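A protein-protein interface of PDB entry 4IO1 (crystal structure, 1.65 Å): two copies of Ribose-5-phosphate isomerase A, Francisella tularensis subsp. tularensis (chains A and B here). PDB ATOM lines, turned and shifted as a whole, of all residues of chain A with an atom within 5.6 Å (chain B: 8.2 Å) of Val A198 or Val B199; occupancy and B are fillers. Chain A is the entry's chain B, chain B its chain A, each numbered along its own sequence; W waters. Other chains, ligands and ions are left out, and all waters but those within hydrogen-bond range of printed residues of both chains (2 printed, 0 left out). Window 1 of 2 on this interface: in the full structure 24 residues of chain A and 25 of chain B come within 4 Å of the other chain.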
ATOM      1  N   ILE A 139     -34.858  -4.914 -19.722  1.00  0.00           N
ATOM      2  CA  ILE A 139     -33.419  -5.090 -19.677  1.00  0.00           C
ATOM      3  C   ILE A 139     -32.819  -4.180 -20.747  1.00  0.00           C
ATOM      4  O   ILE A 139     -33.152  -4.291 -21.924  1.00  0.00           O
ATOM      5  CB  ILE A 139     -33.017  -6.546 -19.936  1.00  0.00           C
ATOM      6  CG1 ILE A 139     -33.762  -7.479 -18.949  1.00  0.00           C
ATOM      7  CG2 ILE A 139     -31.506  -6.655 -19.828  1.00  0.00           C
ATOM      8  CD1 ILE A 139     -33.409  -8.899 -19.059  1.00  0.00           C
ATOM      9  N   GLU A 140     -31.957  -3.258 -20.327  1.00  0.00           N
ATOM     10  CA  GLU A 140     -31.212  -2.394 -21.258  1.00  0.00           C
ATOM     11  C   GLU A 140     -29.950  -3.096 -21.727  1.00  0.00           C
ATOM     12  O   GLU A 140     -29.202  -3.632 -20.900  1.00  0.00           O
ATOM     13  CB  GLU A 140     -30.877  -1.041 -20.611  1.00  0.00           C
ATOM     14  CG  GLU A 140     -30.051  -0.110 -21.486  1.00  0.00           C
ATOM     15  CD  GLU A 140     -30.013   1.328 -20.965  1.00  0.00           C
ATOM     16  OE1 GLU A 140     -30.802   1.648 -20.032  1.00  0.00           O
ATOM     17  OE2 GLU A 140     -29.237   2.129 -21.501  1.00  0.00           O
ATOM     18  N   VAL A 141     -29.749  -3.114 -23.035  1.00  0.00           N
ATOM     19  CA  VAL A 141     -28.687  -3.894 -23.647  1.00  0.00           C
ATOM     20  C   VAL A 141     -27.897  -3.098 -24.687  1.00  0.00           C
ATOM     21  O   VAL A 141     -28.428  -2.243 -25.409  1.00  0.00           O
ATOM     22  CB  VAL A 141     -29.224  -5.216 -24.284  1.00  0.00           C
ATOM     23  CG1 VAL A 141     -30.030  -6.034 -23.246  1.00  0.00           C
ATOM     24  CG2 VAL A 141     -30.026  -4.945 -25.503  1.00  0.00           C
ATOM     25  N   ILE A 142     -26.617  -3.378 -24.745  1.00  0.00           N
ATOM     26  CA  ILE A 142     -25.791  -2.868 -25.816  1.00  0.00           C
ATOM     27  C   ILE A 142     -26.343  -3.374 -27.143  1.00  0.00           C
ATOM     28  O   ILE A 142     -26.547  -4.581 -27.295  1.00  0.00           O
ATOM     29  CB  ILE A 142     -24.317  -3.344 -25.641  1.00  0.00           C
ATOM     30  CG1 ILE A 142     -23.673  -2.805 -24.342  1.00  0.00           C
ATOM     31  CG2 ILE A 142     -23.491  -2.960 -26.834  1.00  0.00           C
ATOM     32  CD1 ILE A 142     -23.493  -1.308 -24.287  1.00  0.00           C
ATOM     33  N   ILE A 149     -28.147 -11.757 -26.351  1.00  0.00           N
ATOM     34  CA  ILE A 149     -28.796 -11.702 -25.017  1.00  0.00           C
ATOM     35  C   ILE A 149     -30.189 -12.301 -25.041  1.00  0.00           C
ATOM     36  O   ILE A 149     -30.561 -13.065 -24.144  1.00  0.00           O
ATOM     37  CB  ILE A 149     -28.849 -10.276 -24.498  1.00  0.00           C
ATOM     38  CG1 ILE A 149     -27.421  -9.746 -24.254  1.00  0.00           C
ATOM     39  CG2 ILE A 149     -29.694 -10.178 -23.198  1.00  0.00           C
ATOM     40  CD1 ILE A 149     -27.284  -8.277 -24.075  1.00  0.00           C
ATOM     41  N   LEU A 192     -28.742 -12.084 -14.531  1.00  0.00           N
ATOM     42  CA  LEU A 192     -28.918 -11.171 -15.650  1.00  0.00           C
ATOM     43  C   LEU A 192     -27.744 -10.178 -15.747  1.00  0.00           C
ATOM     44  O   LEU A 192     -27.260  -9.899 -16.843  1.00  0.00           O
ATOM     45  CB  LEU A 192     -30.243 -10.455 -15.512  1.00  0.00           C
ATOM     46  CG  LEU A 192     -31.488 -11.317 -15.696  1.00  0.00           C
ATOM     47  CD1 LEU A 192     -32.739 -10.451 -15.517  1.00  0.00           C
ATOM     48  CD2 LEU A 192     -31.526 -11.968 -17.064  1.00  0.00           C
ATOM     49  N   ASN A 193     -27.231  -9.739 -14.587  1.00  0.00           N
ATOM     50  CA  ASN A 193     -26.044  -8.881 -14.496  1.00  0.00           C
ATOM     51  C   ASN A 193     -24.802  -9.499 -15.159  1.00  0.00           C
ATOM     52  O   ASN A 193     -23.895  -8.774 -15.560  1.00  0.00           O
ATOM     53  CB  ASN A 193     -25.714  -8.491 -13.072  1.00  0.00           C
ATOM     54  CG  ASN A 193     -26.696  -7.492 -12.484  1.00  0.00           C
ATOM     55  OD1 ASN A 193     -27.427  -6.844 -13.226  1.00  0.00           O
ATOM     56  ND2 ASN A 193     -26.696  -7.340 -11.154  1.00  0.00           N
ATOM     57  N   ILE A 195     -24.779 -11.534 -17.838  1.00  0.00           N
ATOM     58  CA  ILE A 195     -24.900 -11.745 -19.262  1.00  0.00           C
ATOM     59  C   ILE A 195     -24.157 -10.613 -19.964  1.00  0.00           C
ATOM     60  O   ILE A 195     -24.501  -9.429 -19.782  1.00  0.00           O
ATOM     61  CB  ILE A 195     -26.352 -11.845 -19.751  1.00  0.00           C
ATOM     62  CG1 ILE A 195     -27.102 -12.941 -19.012  1.00  0.00           C
ATOM     63  CG2 ILE A 195     -26.418 -12.070 -21.302  1.00  0.00           C
ATOM     64  CD1 ILE A 195     -28.537 -13.005 -19.341  1.00  0.00           C
ATOM     65  N   THR A 196     -23.176 -10.927 -20.792  1.00  0.00           N
ATOM     66  CA  THR A 196     -22.405  -9.903 -21.456  1.00  0.00           C
ATOM     67  C   THR A 196     -23.242  -9.041 -22.378  1.00  0.00           C
ATOM     68  O   THR A 196     -23.975  -9.549 -23.227  1.00  0.00           O
ATOM     69  CB  THR A 196     -21.267 -10.548 -22.312  1.00  0.00           C
ATOM     70  OG1 THR A 196     -20.553 -11.463 -21.480  1.00  0.00           O
ATOM     71  CG2 THR A 196     -20.352  -9.515 -22.804  1.00  0.00           C
ATOM     72  N   GLY A 197     -23.145  -7.735 -22.184  1.00  0.00           N
ATOM     73  CA  GLY A 197     -23.891  -6.805 -22.968  1.00  0.00           C
ATOM     74  C   GLY A 197     -25.103  -6.262 -22.272  1.00  0.00           C
ATOM     75  O   GLY A 197     -25.728  -5.277 -22.751  1.00  0.00           O
ATOM     76  N   VAL A 198     -25.489  -6.895 -21.171  1.00  0.00           N
ATOM     77  CA  VAL A 198     -26.552  -6.328 -20.317  1.00  0.00           C
ATOM     78  C   VAL A 198     -26.001  -5.124 -19.578  1.00  0.00           C
ATOM     79  O   VAL A 198     -24.933  -5.198 -18.944  1.00  0.00           O
ATOM     80  CB  VAL A 198     -27.172  -7.379 -19.339  1.00  0.00           C
ATOM     81  CG1 VAL A 198     -28.070  -6.650 -18.277  1.00  0.00           C
ATOM     82  CG2 VAL A 198     -27.876  -8.499 -20.105  1.00  0.00           C
ATOM     83  N   VAL A 199     -26.653  -3.978 -19.723  1.00  0.00           N
ATOM     84  CA  VAL A 199     -26.277  -2.764 -19.017  1.00  0.00           C
ATOM     85  C   VAL A 199     -26.950  -2.712 -17.637  1.00  0.00           C
ATOM     86  O   VAL A 199     -26.280  -2.634 -16.594  1.00  0.00           O
ATOM     87  CB  VAL A 199     -26.625  -1.535 -19.853  1.00  0.00           C
ATOM     88  CG1 VAL A 199     -26.390  -0.260 -19.082  1.00  0.00           C
ATOM     89  CG2 VAL A 199     -25.830  -1.549 -21.185  1.00  0.00           C
ATOM     90  N   THR A 200     -28.266  -2.866 -17.650  1.00  0.00           N
ATOM     91  CA  THR A 200     -29.095  -2.772 -16.474  1.00  0.00           C
ATOM     92  C   THR A 200     -30.296  -3.724 -16.631  1.00  0.00           C
ATOM     93  O   THR A 200     -30.791  -3.933 -17.754  1.00  0.00           O
ATOM     94  CB  THR A 200     -29.626  -1.319 -16.351  1.00  0.00           C
ATOM     95  OG1 THR A 200     -28.519  -0.405 -16.429  1.00  0.00           O
ATOM     96  CG2 THR A 200     -30.364  -1.121 -15.055  1.00  0.00           C
ATOM     97  N   ASN A 201     -30.750  -4.335 -15.542  1.00  0.00           N
ATOM     98  CA  ASN A 201     -32.023  -5.007 -15.589  1.00  0.00           C
ATOM     99  C   ASN A 201     -32.958  -4.392 -14.554  1.00  0.00           C
ATOM    100  O   ASN A 201     -32.500  -3.755 -13.596  1.00  0.00           O
ATOM    101  CB  ASN A 201     -31.891  -6.521 -15.431  1.00  0.00           C
ATOM    102  CG  ASN A 201     -31.497  -6.950 -14.031  1.00  0.00           C
ATOM    103  OD1 ASN A 201     -32.336  -6.943 -13.109  1.00  0.00           O
ATOM    104  ND2 ASN A 201     -30.222  -7.364 -13.854  1.00  0.00           N
ATOM    105  N   LEU B 106     -13.279  -2.993 -24.671  1.00  0.00           N
ATOM    106  CA  LEU B 106     -13.550  -4.231 -23.929  1.00  0.00           C
ATOM    107  C   LEU B 106     -15.002  -4.690 -24.064  1.00  0.00           C
ATOM    108  O   LEU B 106     -15.253  -5.899 -24.074  1.00  0.00           O
ATOM    109  CB  LEU B 106     -13.169  -4.157 -22.445  1.00  0.00           C
ATOM    110  CG  LEU B 106     -13.865  -3.133 -21.593  1.00  0.00           C
ATOM    111  CD1 LEU B 106     -13.713  -3.497 -20.116  1.00  0.00           C
ATOM    112  CD2 LEU B 106     -13.337  -1.682 -21.837  1.00  0.00           C
ATOM    113  N   THR B 107     -15.951  -3.768 -24.145  1.00  0.00           N
ATOM    114  CA  THR B 107     -17.368  -4.177 -24.178  1.00  0.00           C
ATOM    115  C   THR B 107     -17.723  -4.991 -25.417  1.00  0.00           C
ATOM    116  O   THR B 107     -18.222  -6.156 -25.303  1.00  0.00           O
ATOM    117  CB  THR B 107     -18.329  -3.002 -23.981  1.00  0.00           C
ATOM    118  OG1 THR B 107     -18.156  -2.481 -22.656  1.00  0.00           O
ATOM    119  CG2 THR B 107     -19.770  -3.384 -24.216  1.00  0.00           C
ATOM    120  N   ARG B 108     -17.448  -4.454 -26.588  1.00  0.00           N
ATOM    121  CA  ARG B 108     -17.732  -5.188 -27.850  1.00  0.00           C
ATOM    122  C   ARG B 108     -16.845  -6.447 -27.976  1.00  0.00           C
ATOM    123  O   ARG B 108     -17.298  -7.458 -28.492  1.00  0.00           O
ATOM    124  CB  ARG B 108     -17.696  -4.282 -29.056  1.00  0.00           C
ATOM    125  CG  ARG B 108     -18.753  -3.239 -28.994  1.00  0.00           C
ATOM    126  CD  ARG B 108     -18.746  -2.387 -30.245  1.00  0.00           C
ATOM    127  NE  ARG B 108     -19.652  -1.259 -30.158  1.00  0.00           N
ATOM    128  CZ  ARG B 108     -19.895  -0.440 -31.154  1.00  0.00           C
ATOM    129  NH1 ARG B 108     -19.337  -0.629 -32.344  1.00  0.00           N
ATOM    130  NH2 ARG B 108     -20.692   0.593 -30.937  1.00  0.00           N
ATOM    131  N   LYS B 110     -15.876  -8.323 -25.398  1.00  0.00           N
ATOM    132  CA  LYS B 110     -16.427  -9.345 -24.545  1.00  0.00           C
ATOM    133  C   LYS B 110     -17.726  -9.948 -25.133  1.00  0.00           C
ATOM    134  O   LYS B 110     -18.010 -11.145 -25.014  1.00  0.00           O
ATOM    135  CB  LYS B 110     -16.665  -8.799 -23.143  1.00  0.00           C
ATOM    136  CG  LYS B 110     -16.662  -9.874 -22.089  1.00  0.00           C
ATOM    137  CD  LYS B 110     -16.641  -9.196 -20.702  1.00  0.00           C
ATOM    138  CE  LYS B 110     -15.832  -9.853 -19.695  1.00  0.00           C
ATOM    139  NZ  LYS B 110     -15.863  -9.281 -18.335  1.00  0.00           N
ATOM    140  N   ILE B 111     -18.506  -9.105 -25.805  1.00  0.00           N
ATOM    141  CA  ILE B 111     -19.686  -9.573 -26.523  1.00  0.00           C
ATOM    142  C   ILE B 111     -19.323 -10.542 -27.639  1.00  0.00           C
ATOM    143  O   ILE B 111     -19.924 -11.652 -27.752  1.00  0.00           O
ATOM    144  CB  ILE B 111     -20.496  -8.359 -27.079  1.00  0.00           C
ATOM    145  CG1 ILE B 111     -21.068  -7.530 -25.916  1.00  0.00           C
ATOM    146  CG2 ILE B 111     -21.579  -8.849 -28.012  1.00  0.00           C
ATOM    147  CD1 ILE B 111     -21.516  -6.116 -26.354  1.00  0.00           C
ATOM    148  N   ILE B 139     -12.568  -0.616 -16.776  1.00  0.00           N
ATOM    149  CA  ILE B 139     -13.995  -0.856 -16.559  1.00  0.00           C
ATOM    150  C   ILE B 139     -14.749   0.229 -17.324  1.00  0.00           C
ATOM    151  O   ILE B 139     -14.496   1.425 -17.131  1.00  0.00           O
ATOM    152  CB  ILE B 139     -14.366  -0.765 -15.088  1.00  0.00           C
ATOM    153  CG1 ILE B 139     -13.559  -1.800 -14.251  1.00  0.00           C
ATOM    154  CG2 ILE B 139     -15.840  -1.035 -14.885  1.00  0.00           C
ATOM    155  CD1 ILE B 139     -13.932  -1.741 -12.794  1.00  0.00           C
ATOM    156  N   GLU B 140     -15.655  -0.206 -18.199  1.00  0.00           N
ATOM    157  CA  GLU B 140     -16.503   0.737 -18.952  1.00  0.00           C
ATOM    158  C   GLU B 140     -17.707   1.055 -18.096  1.00  0.00           C
ATOM    159  O   GLU B 140     -18.366   0.148 -17.626  1.00  0.00           O
ATOM    160  CB  GLU B 140     -16.927   0.170 -20.284  1.00  0.00           C
ATOM    161  CG  GLU B 140     -17.766   1.150 -21.094  1.00  0.00           C
ATOM    162  CD  GLU B 140     -17.904   0.753 -22.545  1.00  0.00           C
ATOM    163  OE1 GLU B 140     -17.227  -0.171 -23.028  1.00  0.00           O
ATOM    164  OE2 GLU B 140     -18.728   1.404 -23.207  1.00  0.00           O
ATOM    165  N   VAL B 141     -18.024   2.339 -17.943  1.00  0.00           N
ATOM    166  CA  VAL B 141     -19.073   2.764 -17.046  1.00  0.00           C
ATOM    167  C   VAL B 141     -19.976   3.814 -17.715  1.00  0.00           C
ATOM    168  O   VAL B 141     -19.563   4.572 -18.579  1.00  0.00           O
ATOM    169  CB  VAL B 141     -18.543   3.339 -15.700  1.00  0.00           C
ATOM    170  CG1 VAL B 141     -17.642   2.320 -15.004  1.00  0.00           C
ATOM    171  CG2 VAL B 141     -17.814   4.625 -15.836  1.00  0.00           C
ATOM    172  N   ILE B 142     -21.229   3.755 -17.318  1.00  0.00           N
ATOM    173  CA  ILE B 142     -22.204   4.775 -17.702  1.00  0.00           C
ATOM    174  C   ILE B 142     -21.773   6.094 -17.116  1.00  0.00           C
ATOM    175  O   ILE B 142     -21.480   6.196 -15.918  1.00  0.00           O
ATOM    176  CB  ILE B 142     -23.586   4.384 -17.151  1.00  0.00           C
ATOM    177  CG1 ILE B 142     -24.141   3.126 -17.785  1.00  0.00           C
ATOM    178  CG2 ILE B 142     -24.566   5.550 -17.355  1.00  0.00           C
ATOM    179  CD1 ILE B 142     -24.371   3.159 -19.334  1.00  0.00           C
ATOM    180  N   PRO B 143     -21.708   7.139 -17.957  1.00  0.00           N
ATOM    181  CA  PRO B 143     -21.064   8.344 -17.417  1.00  0.00           C
ATOM    182  C   PRO B 143     -21.713   8.915 -16.159  1.00  0.00           C
ATOM    183  O   PRO B 143     -20.994   9.328 -15.263  1.00  0.00           O
ATOM    184  CB  PRO B 143     -21.111   9.322 -18.596  1.00  0.00           C
ATOM    185  CG  PRO B 143     -21.019   8.473 -19.773  1.00  0.00           C
ATOM    186  CD  PRO B 143     -21.806   7.190 -19.422  1.00  0.00           C
ATOM    187  N   ALA B 145     -22.866   7.436 -13.713  1.00  0.00           N
ATOM    188  CA  ALA B 145     -22.561   6.599 -12.566  1.00  0.00           C
ATOM    189  C   ALA B 145     -21.082   6.697 -12.199  1.00  0.00           C
ATOM    190  O   ALA B 145     -20.650   6.038 -11.261  1.00  0.00           O
ATOM    191  CB  ALA B 145     -22.854   5.153 -12.883  1.00  0.00           C
ATOM    192  N   ILE B 149     -19.483   4.743  -8.955  1.00  0.00           N
ATOM    193  CA  ILE B 149     -18.773   3.498  -9.134  1.00  0.00           C
ATOM    194  C   ILE B 149     -17.374   3.656  -8.528  1.00  0.00           C
ATOM    195  O   ILE B 149     -16.868   2.713  -7.884  1.00  0.00           O
ATOM    196  CB  ILE B 149     -18.693   3.156 -10.593  1.00  0.00           C
ATOM    197  CG1 ILE B 149     -20.098   2.778 -11.085  1.00  0.00           C
ATOM    198  CG2 ILE B 149     -17.708   1.993 -10.843  1.00  0.00           C
ATOM    199  CD1 ILE B 149     -20.171   2.621 -12.587  1.00  0.00           C
ATOM    200  N   THR B 168     -15.808   5.617 -25.324  1.00  0.00           N
ATOM    201  CA  THR B 168     -15.871   4.366 -26.025  1.00  0.00           C
ATOM    202  C   THR B 168     -16.808   4.434 -27.225  1.00  0.00           C
ATOM    203  O   THR B 168     -17.598   5.378 -27.360  1.00  0.00           O
ATOM    204  CB  THR B 168     -16.335   3.222 -25.120  1.00  0.00           C
ATOM    205  OG1 THR B 168     -17.729   3.391 -24.847  1.00  0.00           O
ATOM    206  CG2 THR B 168     -15.527   3.231 -23.842  1.00  0.00           C
ATOM    207  N   ASN B 170     -19.366   2.982 -27.538  1.00  0.00           N
ATOM    208  CA  ASN B 170     -20.703   2.897 -27.044  1.00  0.00           C
ATOM    209  C   ASN B 170     -21.173   4.188 -26.355  1.00  0.00           C
ATOM    210  O   ASN B 170     -22.281   4.248 -25.872  1.00  0.00           O
ATOM    211  CB  ASN B 170     -20.865   1.732 -26.089  1.00  0.00           C
ATOM    212  CG  ASN B 170     -20.159   0.501 -26.580  1.00  0.00           C
ATOM    213  OD1 ASN B 170     -20.575  -0.072 -27.573  1.00  0.00           O
ATOM    214  ND2 ASN B 170     -19.052   0.116 -25.921  1.00  0.00           N
ATOM    215  N   GLY B 171     -20.278   5.164 -26.271  1.00  0.00           N
ATOM    216  CA  GLY B 171     -20.594   6.489 -25.719  1.00  0.00           C
ATOM    217  C   GLY B 171     -20.302   6.576 -24.239  1.00  0.00           C
ATOM    218  O   GLY B 171     -20.668   7.531 -23.602  1.00  0.00           O
ATOM    219  N   ASN B 172     -19.628   5.580 -23.684  1.00  0.00           N
ATOM    220  CA  ASN B 172     -19.331   5.593 -22.266  1.00  0.00           C
ATOM    221  C   ASN B 172     -17.905   5.991 -21.945  1.00  0.00           C
ATOM    222  O   ASN B 172     -17.123   6.286 -22.848  1.00  0.00           O
ATOM    223  CB  ASN B 172     -19.629   4.191 -21.710  1.00  0.00           C
ATOM    224  CG  ASN B 172     -21.103   3.818 -21.928  1.00  0.00           C
ATOM    225  OD1 ASN B 172     -21.994   4.631 -21.693  1.00  0.00           O
ATOM    226  ND2 ASN B 172     -21.332   2.649 -22.499  1.00  0.00           N
ATOM    227  N   VAL B 173     -17.574   6.012 -20.661  1.00  0.00           N
ATOM    228  CA  VAL B 173     -16.227   6.377 -20.244  1.00  0.00           C
ATOM    229  C   VAL B 173     -15.584   5.176 -19.547  1.00  0.00           C
ATOM    230  O   VAL B 173     -16.248   4.163 -19.290  1.00  0.00           O
ATOM    231  CB  VAL B 173     -16.162   7.602 -19.361  1.00  0.00           C
ATOM    232  CG1 VAL B 173     -16.733   8.852 -20.114  1.00  0.00           C
ATOM    233  CG2 VAL B 173     -16.903   7.404 -18.089  1.00  0.00           C
ATOM    234  N   LEU B 192     -17.698  -7.248  -9.833  1.00  0.00           N
ATOM    235  CA  LEU B 192     -17.746  -5.956 -10.554  1.00  0.00           C
ATOM    236  C   LEU B 192     -18.981  -5.816 -11.436  1.00  0.00           C
ATOM    237  O   LEU B 192     -19.500  -4.695 -11.629  1.00  0.00           O
ATOM    238  CB  LEU B 192     -16.452  -5.778 -11.384  1.00  0.00           C
ATOM    239  CG  LEU B 192     -15.140  -5.653 -10.586  1.00  0.00           C
ATOM    240  CD1 LEU B 192     -13.938  -5.689 -11.507  1.00  0.00           C
ATOM    241  CD2 LEU B 192     -15.133  -4.401  -9.700  1.00  0.00           C
ATOM    242  N   ASN B 193     -19.461  -6.935 -12.014  1.00  0.00           N
ATOM    243  CA  ASN B 193     -20.690  -6.961 -12.823  1.00  0.00           C
ATOM    244  C   ASN B 193     -21.944  -6.564 -12.028  1.00  0.00           C
ATOM    245  O   ASN B 193     -22.957  -6.170 -12.612  1.00  0.00           O
ATOM    246  CB  ASN B 193     -20.927  -8.310 -13.499  1.00  0.00           C
ATOM    247  CG  ASN B 193     -19.982  -8.583 -14.666  1.00  0.00           C
ATOM    248  OD1 ASN B 193     -19.407  -7.649 -15.224  1.00  0.00           O
ATOM    249  ND2 ASN B 193     -19.848  -9.846 -15.047  1.00  0.00           N
ATOM    250  N   ILE B 195     -22.032  -4.115  -9.832  1.00  0.00           N
ATOM    251  CA  ILE B 195     -22.042  -2.684  -9.533  1.00  0.00           C
ATOM    252  C   ILE B 195     -22.861  -1.914 -10.548  1.00  0.00           C
ATOM    253  O   ILE B 195     -22.572  -1.942 -11.739  1.00  0.00           O
ATOM    254  CB  ILE B 195     -20.596  -2.059  -9.430  1.00  0.00           C
ATOM    255  CG1 ILE B 195     -19.774  -2.822  -8.409  1.00  0.00           C
ATOM    256  CG2 ILE B 195     -20.702  -0.621  -9.073  1.00  0.00           C
ATOM    257  CD1 ILE B 195     -18.312  -2.433  -8.341  1.00  0.00           C
ATOM    258  N   THR B 196     -23.903  -1.211 -10.070  1.00  0.00           N
ATOM    259  CA  THR B 196     -24.802  -0.499 -10.945  1.00  0.00           C
ATOM    260  C   THR B 196     -24.095   0.588 -11.734  1.00  0.00           C
ATOM    261  O   THR B 196     -23.370   1.413 -11.160  1.00  0.00           O
ATOM    262  CB  THR B 196     -25.963   0.119 -10.124  1.00  0.00           C
ATOM    263  OG1 THR B 196     -26.605  -0.954  -9.416  1.00  0.00           O
ATOM    264  CG2 THR B 196     -26.998   0.723 -11.043  1.00  0.00           C
ATOM    265  N   GLY B 197     -24.313   0.578 -13.047  1.00  0.00           N
ATOM    266  CA  GLY B 197     -23.622   1.461 -13.962  1.00  0.00           C
ATOM    267  C   GLY B 197     -22.402   0.887 -14.649  1.00  0.00           C
ATOM    268  O   GLY B 197     -21.871   1.516 -15.586  1.00  0.00           O
ATOM    269  N   VAL B 198     -21.882  -0.264 -14.165  1.00  0.00           N
ATOM    270  CA  VAL B 198     -20.800  -0.925 -14.842  1.00  0.00           C
ATOM    271  C   VAL B 198     -21.367  -1.595 -16.085  1.00  0.00           C
ATOM    272  O   VAL B 198     -22.327  -2.379 -15.998  1.00  0.00           O
ATOM    273  CB  VAL B 198     -20.115  -1.949 -13.933  1.00  0.00           C
ATOM    274  CG1 VAL B 198     -19.157  -2.840 -14.766  1.00  0.00           C
ATOM    275  CG2 VAL B 198     -19.348  -1.257 -12.844  1.00  0.00           C
ATOM    276  N   VAL B 199     -20.823  -1.288 -17.256  1.00  0.00           N
ATOM    277  CA  VAL B 199     -21.214  -1.934 -18.498  1.00  0.00           C
ATOM    278  C   VAL B 199     -20.456  -3.257 -18.665  1.00  0.00           C
ATOM    279  O   VAL B 199     -21.070  -4.309 -18.772  1.00  0.00           O
ATOM    280  CB  VAL B 199     -20.990  -0.985 -19.696  1.00  0.00           C
ATOM    281  CG1 VAL B 199     -21.323  -1.692 -21.020  1.00  0.00           C
ATOM    282  CG2 VAL B 199     -21.841   0.300 -19.529  1.00  0.00           C
ATOM    283  N   THR B 200     -19.128  -3.212 -18.723  1.00  0.00           N
ATOM    284  CA  THR B 200     -18.333  -4.427 -18.606  1.00  0.00           C
ATOM    285  C   THR B 200     -17.023  -4.124 -17.947  1.00  0.00           C
ATOM    286  O   THR B 200     -16.494  -3.029 -18.045  1.00  0.00           O
ATOM    287  CB  THR B 200     -17.983  -5.057 -19.960  1.00  0.00           C
ATOM    288  OG1 THR B 200     -17.359  -6.325 -19.755  1.00  0.00           O
ATOM    289  CG2 THR B 200     -17.014  -4.163 -20.682  1.00  0.00           C
ATOM    290  N   ASN B 201     -16.454  -5.146 -17.338  1.00  0.00           N
ATOM    291  CA  ASN B 201     -15.113  -5.029 -16.738  1.00  0.00           C
ATOM    292  C   ASN B 201     -14.116  -5.860 -17.549  1.00  0.00           C
ATOM    293  O   ASN B 201     -14.508  -6.783 -18.287  1.00  0.00           O
ATOM    294  CB  ASN B 201     -15.079  -5.410 -15.239  1.00  0.00           C
ATOM    295  CG  ASN B 201     -15.308  -6.878 -15.011  1.00  0.00           C
ATOM    296  OD1 ASN B 201     -14.387  -7.653 -15.185  1.00  0.00           O
ATOM    297  ND2 ASN B 201     -16.548  -7.271 -14.666  1.00  0.00           N
ATOM    298  N   GLY B 202     -12.847  -5.513 -17.439  1.00  0.00           N
ATOM    299  CA  GLY B 202     -11.805  -6.079 -18.300  1.00  0.00           C
ATOM    300  C   GLY B 202     -11.292  -7.448 -17.920  1.00  0.00           C
ATOM    301  O   GLY B 202     -10.386  -7.918 -18.586  1.00  0.00           O
HETATM  302  O   HOH W   1     -24.694  -1.842 -14.583  1.00  0.00           O
HETATM  303  O   HOH W   2     -22.626  -6.342 -19.707  1.00  0.00           O
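The backbone carbonyl oxygen (O) of Glu A140 lies within hydrogen-bond range of the backbone NH (N) of Val A199 (2.8 Å). The backbone NH of Ile A142 is in hydrogen-bond range of the backbone carbonyl oxygen of Gly A197 (2.9 Å). The backbone NH (N) of Ile B142 sits at hydrogen-bond distance from the backbone carbonyl oxygen (O) of Gly B197, 2.9 Å away. O of Glu B140 sits at hydrogen-bond distance from N of Val B199 (2.9 Å). The side-chain amide nitrogen of Asn B201 sits at hydrogen-bond distance from the side-chain amide oxygen of Asn B193. OE1 of Glu B140 is in hydrogen-bond range of OG1 of Thr B107 (2.5 Å).
Among the printed residues, merely in contact across the chains: Thr A196 with Lys B110 (3.5 Å), Thr A196 with Ile B111 (3.5 Å), Asn A193 with Asn B193 (3.6 Å), Ile A142 with Ile B111 (3.8 Å), Ile A142 with Val B199 (3.9 Å), Ile A142 with Thr B107 (3.9 Å), Val A198 with Val B199 (3.97 Å) and Val A199 with Ile B142 (3.98 Å).
Printed residues of chain B within 4 Å of Ile A142: Thr B107 (3.9 Å), Ile B111 (3.8 Å) and Val B199 (3.9 Å). No residue of chain B comes within 4 Å of Gly A197. Val A198 touches one residue of chain B. Of the printed residues of chain A, Lys B110 touches Thr A196. Of the printed residues of chain A, Ile B111 touches Ile A142 (3.8 Å) and Thr A196 (3.5 Å). Printed residues of chain A within 4 Å of Asn B193: Asn A193. Gly B202 touches none of the printed residues of chain A. The nearest printed residue of chain B that does not touch Val A199 is Val B198 (4.01 Å).
Printed residues of chain A that touch a printed residue of chain B: Ile A142, Asn A193, Thr A196, Val A198 and Val A199. Hydrophobic or aromatic side chains of chain A that line the printed part of chain B: Ile A142 and Val A199. Among the printed residues, no Asp or Glu carboxylate lies within 4 Å of a Lys or Arg side-chain nitrogen of the other chain.
Ile A142 touches Val B199, and with the chains exchanged Val A199 touches Ile B142. Asn B193 touches its own counterpart, Asn A193. Val A198 touches Val B199, but with the chains exchanged Val A199 does not touch Val B198 (4.01 Å). 14 positions are printed for both chains. Of the 8 pairs that touch across the chains among the printed residues, 3 have their exchanged pair printed and touching as well.
Water W1 lies within hydrogen-bond range of the backbone carbonyl oxygen of Val A199 (2.7 Å), the backbone carbonyl oxygen of Val B198 (2.8 Å) and the backbone NH of Gly B197 (2.9 Å). Water W2 lies within hydrogen-bond range of the backbone carbonyl oxygen (O) of Val A198, the backbone carbonyl oxygen (O) of Val B199 and the backbone NH (N) of Gly A197.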
